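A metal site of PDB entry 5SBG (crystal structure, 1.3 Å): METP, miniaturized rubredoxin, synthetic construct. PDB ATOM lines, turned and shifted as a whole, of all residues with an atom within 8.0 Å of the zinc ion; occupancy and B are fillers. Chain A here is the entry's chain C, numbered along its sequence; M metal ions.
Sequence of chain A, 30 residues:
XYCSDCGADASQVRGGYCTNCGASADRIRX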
ATOM      1  N   TYR A   2       2.390 -29.873  16.713  1.00  0.00           N
ATOM      2  CA  TYR A   2       1.270 -29.159  17.328  1.00  0.00           C
ATOM      3  C   TYR A   2       1.532 -27.654  17.302  1.00  0.00           C
ATOM      4  O   TYR A   2       2.683 -27.208  17.234  1.00  0.00           O
ATOM      5  CB  TYR A   2       1.090 -29.623  18.785  1.00  0.00           C
ATOM      6  CG  TYR A   2       2.285 -29.233  19.644  1.00  0.00           C
ATOM      7  CD1 TYR A   2       3.475 -29.959  19.608  1.00  0.00           C
ATOM      8  CD2 TYR A   2       2.242 -28.105  20.449  1.00  0.00           C
ATOM      9  CE1 TYR A   2       4.568 -29.571  20.353  1.00  0.00           C
ATOM     10  CE2 TYR A   2       3.331 -27.724  21.184  1.00  0.00           C
ATOM     11  CZ  TYR A   2       4.493 -28.457  21.136  1.00  0.00           C
ATOM     12  OH  TYR A   2       5.573 -28.048  21.875  1.00  0.00           O
ATOM     13  N   CYS A   3       0.456 -26.893  17.376  1.00  0.00           N
ATOM     14  CA  CYS A   3       0.537 -25.444  17.552  1.00  0.00           C
ATOM     15  C   CYS A   3       0.801 -25.136  19.018  1.00  0.00           C
ATOM     16  O   CYS A   3       0.017 -25.525  19.893  1.00  0.00           O
ATOM     17  CB  CYS A   3      -0.765 -24.764  17.140  1.00  0.00           C
ATOM     18  SG  CYS A   3      -0.709 -22.951  17.415  1.00  0.00           S
ATOM     19  N   SER A   4       1.909 -24.465  19.288  1.00  0.00           N
ATOM     20  CA  SER A   4       2.232 -24.162  20.673  1.00  0.00           C
ATOM     21  C   SER A   4       1.255 -23.181  21.299  1.00  0.00           C
ATOM     22  O   SER A   4       1.094 -23.181  22.519  1.00  0.00           O
ATOM     23  CB  SER A   4       3.661 -23.676  20.809  1.00  0.00           C
ATOM     24  OG  SER A   4       3.920 -22.488  20.101  1.00  0.00           O
ATOM     25  N   ASP A   5       0.572 -22.357  20.483  1.00  0.00           N
ATOM     26  CA  ASP A   5      -0.343 -21.373  21.039  1.00  0.00           C
ATOM     27  C   ASP A   5      -1.701 -21.967  21.433  1.00  0.00           C
ATOM     28  O   ASP A   5      -2.295 -21.545  22.424  1.00  0.00           O
ATOM     29  CB  ASP A   5      -0.550 -20.222  20.055  1.00  0.00           C
ATOM     30  CG  ASP A   5       0.460 -19.118  20.214  1.00  0.00           C
ATOM     31  OD1 ASP A   5       1.415 -19.254  21.011  1.00  0.00           O
ATOM     32  OD2 ASP A   5       0.280 -18.098  19.532  1.00  0.00           O
ATOM     33  N   CYS A   6      -2.226 -22.930  20.674  1.00  0.00           N
ATOM     34  CA  CYS A   6      -3.567 -23.446  20.920  1.00  0.00           C
ATOM     35  C   CYS A   6      -3.660 -24.968  21.035  1.00  0.00           C
ATOM     36  O   CYS A   6      -4.733 -25.471  21.408  1.00  0.00           O
ATOM     37  CB  CYS A   6      -4.564 -22.958  19.863  1.00  0.00           C
ATOM     38  SG  CYS A   6      -4.402 -23.783  18.241  1.00  0.00           S
ATOM     39  N   GLY A   7      -2.609 -25.707  20.680  1.00  0.00           N
ATOM     40  CA  GLY A   7      -2.619 -27.158  20.790  1.00  0.00           C
ATOM     41  C   GLY A   7      -3.100 -27.892  19.556  1.00  0.00           C
ATOM     42  O   GLY A   7      -3.085 -29.122  19.535  1.00  0.00           O
ATOM     43  N   ALA A   8      -3.529 -27.152  18.522  1.00  0.00           N
ATOM     44  CA  ALA A   8      -4.066 -27.808  17.344  1.00  0.00           C
ATOM     45  C   ALA A   8      -3.018 -28.694  16.685  1.00  0.00           C
ATOM     46  O   ALA A   8      -1.815 -28.428  16.747  1.00  0.00           O
ATOM     47  CB  ALA A   8      -4.503 -26.726  16.355  1.00  0.00           C
ATOM     48  N   ASP A   9      -3.484 -29.760  16.050  1.00  0.00           N
ATOM     49  CA  ASP A   9      -2.579 -30.646  15.319  1.00  0.00           C
ATOM     50  C   ASP A   9      -1.917 -29.926  14.159  1.00  0.00           C
ATOM     51  O   ASP A   9      -2.519 -29.086  13.510  1.00  0.00           O
ATOM     52  CB  ASP A   9      -3.348 -31.828  14.761  1.00  0.00           C
ATOM     53  CG  ASP A   9      -2.445 -32.894  14.188  1.00  0.00           C
ATOM     54  OD1 ASP A   9      -1.937 -33.722  14.982  1.00  0.00           O
ATOM     55  OD2 ASP A   9      -2.227 -32.911  12.955  1.00  0.00           O
ATOM     56  N   AIB A  10      -0.623 -30.192  13.957  1.00  0.00           N
ATOM     57  CA  AIB A  10       0.124 -29.602  12.875  1.00  0.00           C
ATOM     58  C   AIB A  10      -0.493 -29.707  11.475  1.00  0.00           C
ATOM     59  O   AIB A  10      -0.241 -28.909  10.591  1.00  0.00           O
ATOM     60  CB1 AIB A  10       1.528 -30.212  12.761  1.00  0.00           C
ATOM     61  CB2 AIB A  10       0.300 -28.108  13.203  1.00  0.00           C
ATOM     62  N   GLN A  12      -3.229 -28.863  10.695  1.00  0.00           N
ATOM     63  CA  GLN A  12      -4.169 -27.763  10.550  1.00  0.00           C
ATOM     64  C   GLN A  12      -3.490 -26.426  10.211  1.00  0.00           C
ATOM     65  O   GLN A  12      -4.119 -25.364  10.337  1.00  0.00           O
ATOM     66  CB  GLN A  12      -5.040 -27.611  11.803  1.00  0.00           C
ATOM     67  CG  GLN A  12      -5.934 -28.812  12.106  1.00  0.00           C
ATOM     68  CD  GLN A  12      -6.505 -29.457  10.857  1.00  0.00           C
ATOM     69  OE1 GLN A  12      -7.312 -28.862  10.139  1.00  0.00           O
ATOM     70  NE2 GLN A  12      -6.069 -30.684  10.576  1.00  0.00           N
ATOM     71  N   VAL A  13      -2.254 -26.435   9.752  1.00  0.00           N
ATOM     72  CA  VAL A  13      -1.557 -25.210   9.402  1.00  0.00           C
ATOM     73  C   VAL A  13      -1.614 -25.035   7.898  1.00  0.00           C
ATOM     74  O   VAL A  13      -1.387 -25.996   7.146  1.00  0.00           O
ATOM     75  CB  VAL A  13      -0.105 -25.238   9.909  1.00  0.00           C
ATOM     76  CG1 VAL A  13       0.642 -24.027   9.434  1.00  0.00           C
ATOM     77  CG2 VAL A  13      -0.107 -25.288  11.406  1.00  0.00           C
ATOM     78  N   TYR A  17      -0.104 -19.946   8.648  1.00  0.00           N
ATOM     79  CA  TYR A  17      -0.785 -19.714   9.908  1.00  0.00           C
ATOM     80  C   TYR A  17      -1.448 -20.970  10.436  1.00  0.00           C
ATOM     81  O   TYR A  17      -1.916 -21.825   9.668  1.00  0.00           O
ATOM     82  CB  TYR A  17      -1.874 -18.642   9.787  1.00  0.00           C
ATOM     83  CG  TYR A  17      -1.347 -17.314   9.333  1.00  0.00           C
ATOM     84  CD1 TYR A  17      -0.900 -16.373  10.250  1.00  0.00           C
ATOM     85  CD2 TYR A  17      -1.266 -17.013   7.986  1.00  0.00           C
ATOM     86  CE1 TYR A  17      -0.395 -15.181   9.840  1.00  0.00           C
ATOM     87  CE2 TYR A  17      -0.757 -15.785   7.553  1.00  0.00           C
ATOM     88  CZ  TYR A  17      -0.337 -14.880   8.493  1.00  0.00           C
ATOM     89  OH  TYR A  17       0.173 -13.659   8.100  1.00  0.00           O
ATOM     90  N   CYS A  18      -1.527 -21.072  11.770  1.00  0.00           N
ATOM     91  CA  CYS A  18      -2.450 -22.036  12.362  1.00  0.00           C
ATOM     92  C   CYS A  18      -3.882 -21.658  12.024  1.00  0.00           C
ATOM     93  O   CYS A  18      -4.321 -20.523  12.308  1.00  0.00           O
ATOM     94  CB  CYS A  18      -2.258 -22.069  13.884  1.00  0.00           C
ATOM     95  SG  CYS A  18      -3.471 -23.107  14.724  1.00  0.00           S
ATOM     96  N   THR A  19      -4.620 -22.574  11.384  1.00  0.00           N
ATOM     97  CA  THR A  19      -5.973 -22.223  10.960  1.00  0.00           C
ATOM     98  C   THR A  19      -6.969 -22.204  12.116  1.00  0.00           C
ATOM     99  O   THR A  19      -8.129 -21.828  11.912  1.00  0.00           O
ATOM    100  CB  THR A  19      -6.473 -23.144   9.854  1.00  0.00           C
ATOM    101  OG1 THR A  19      -6.579 -24.482  10.361  1.00  0.00           O
ATOM    102  CG2 THR A  19      -5.582 -23.109   8.596  1.00  0.00           C
ATOM    103  N   ASN A  20      -6.543 -22.615  13.314  1.00  0.00           N
ATOM    104  CA  ASN A  20      -7.411 -22.503  14.467  1.00  0.00           C
ATOM    105  C   ASN A  20      -7.245 -21.158  15.174  1.00  0.00           C
ATOM    106  O   ASN A  20      -8.216 -20.433  15.374  1.00  0.00           O
ATOM    107  CB  ASN A  20      -7.204 -23.652  15.441  1.00  0.00           C
ATOM    108  CG  ASN A  20      -8.168 -23.614  16.590  1.00  0.00           C
ATOM    109  OD1 ASN A  20      -9.388 -23.588  16.391  1.00  0.00           O
ATOM    110  ND2 ASN A  20      -7.639 -23.599  17.809  1.00  0.00           N
ATOM    111  N   CYS A  21      -6.027 -20.821  15.595  1.00  0.00           N
ATOM    112  CA  CYS A  21      -5.805 -19.645  16.412  1.00  0.00           C
ATOM    113  C   CYS A  21      -5.139 -18.481  15.694  1.00  0.00           C
ATOM    114  O   CYS A  21      -5.013 -17.404  16.287  1.00  0.00           O
ATOM    115  CB  CYS A  21      -4.974 -20.008  17.653  1.00  0.00           C
ATOM    116  SG  CYS A  21      -3.231 -20.244  17.339  1.00  0.00           S
ATOM    117  N   GLY A  22      -4.734 -18.655  14.442  1.00  0.00           N
ATOM    118  CA  GLY A  22      -4.090 -17.609  13.681  1.00  0.00           C
ATOM    119  C   GLY A  22      -2.647 -17.365  14.005  1.00  0.00           C
ATOM    120  O   GLY A  22      -2.060 -16.406  13.491  1.00  0.00           O
ATOM    121  N   ALA A  23      -2.020 -18.247  14.799  1.00  0.00           N
ATOM    122  CA  ALA A  23      -0.602 -18.088  15.097  1.00  0.00           C
ATOM    123  C   ALA A  23       0.241 -18.163  13.828  1.00  0.00           C
ATOM    124  O   ALA A  23      -0.088 -18.895  12.871  1.00  0.00           O
ATOM    125  CB  ALA A  23      -0.156 -19.193  16.061  1.00  0.00           C
ATOM    126  N   SER A  24       1.317 -17.398  13.821  1.00  0.00           N
ATOM    127  CA  SER A  24       2.288 -17.500  12.741  1.00  0.00           C
ATOM    128  C   SER A  24       2.924 -18.884  12.707  1.00  0.00           C
ATOM    129  O   SER A  24       2.989 -19.582  13.724  1.00  0.00           O
ATOM    130  CB  SER A  24       3.359 -16.424  12.875  1.00  0.00           C
ATOM    131  OG  SER A  24       4.015 -16.518  14.115  1.00  0.00           O
ATOM    132  N   ARG A  27       5.124 -20.795  15.294  1.00  0.00           N
ATOM    133  CA  ARG A  27       4.630 -21.306  16.566  1.00  0.00           C
ATOM    134  C   ARG A  27       4.337 -22.797  16.554  1.00  0.00           C
ATOM    135  O   ARG A  27       4.069 -23.378  17.611  1.00  0.00           O
ATOM    136  CB  ARG A  27       3.374 -20.538  16.997  1.00  0.00           C
ATOM    137  CG  ARG A  27       3.620 -19.301  17.846  1.00  0.00           C
ATOM    138  CD  ARG A  27       4.584 -18.321  17.237  1.00  0.00           C
ATOM    139  NE  ARG A  27       4.603 -17.072  18.016  1.00  0.00           N
ATOM    140  CZ  ARG A  27       5.493 -16.096  17.864  1.00  0.00           C
ATOM    141  NH1 ARG A  27       6.468 -16.206  16.996  1.00  0.00           N
ATOM    142  NH2 ARG A  27       5.400 -15.012  18.620  1.00  0.00           N
ATOM    143  N   ILE A  28       4.387 -23.441  15.383  1.00  0.00           N
ATOM    144  CA  ILE A  28       4.221 -24.893  15.287  1.00  0.00           C
ATOM    145  C   ILE A  28       5.505 -25.552  15.764  1.00  0.00           C
ATOM    146  O   ILE A  28       6.606 -25.145  15.383  1.00  0.00           O
ATOM    147  CB  ILE A  28       3.917 -25.300  13.843  1.00  0.00           C
ATOM    148  CG1 ILE A  28       2.731 -24.508  13.301  1.00  0.00           C
ATOM    149  CG2 ILE A  28       3.682 -26.796  13.748  1.00  0.00           C
ATOM    150  CD1 ILE A  28       1.478 -24.594  14.118  1.00  0.00           C
HETATM  151 ZN    ZN M   1      -2.953 -22.501  16.972  1.00  0.00          ZN
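SG of Cys 21 lies close to N of Ala 23, at 3.5 Å.
N of Ala 8 lies close to SG of Cys 6 (3.5 Å).
SG of Cys 6 lies close to ND2 of Asn 20 (3.3 Å).
The side-chain sulfur (SG) of Cys 3 lies close to the backbone NH (N) of Asp 5, 3.4 Å away.
O of Ala 8 lies within hydrogen-bond range of N of Cys 3 (2.8 Å).
The backbone NH (N) of Cys 18 lies within hydrogen-bond range of the backbone carbonyl oxygen (O) of Ala 23 (2.8 Å).
SG of Cys 18 lies close to N of Asn 20, 3.4 Å away.
Four residues have an atom within 4 Å of the zinc ion: Cys 3, Cys 6, Cys 18 and Cys 21.
The nearest printed residue that does not touch the zinc ion is Ala 23 (4.4 Å).
SG of Cys 21 binds the zinc ion, 2.3 Å away.
The side-chain sulfur (SG) of Cys 6 binds the zinc ion (2.3 Å).
SG of Cys 3 binds the zinc ion, 2.3 Å away.
The side-chain sulfur (SG) of Cys 18 is bound to the zinc ion.
The zinc ion has four donor atoms within binding distance.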
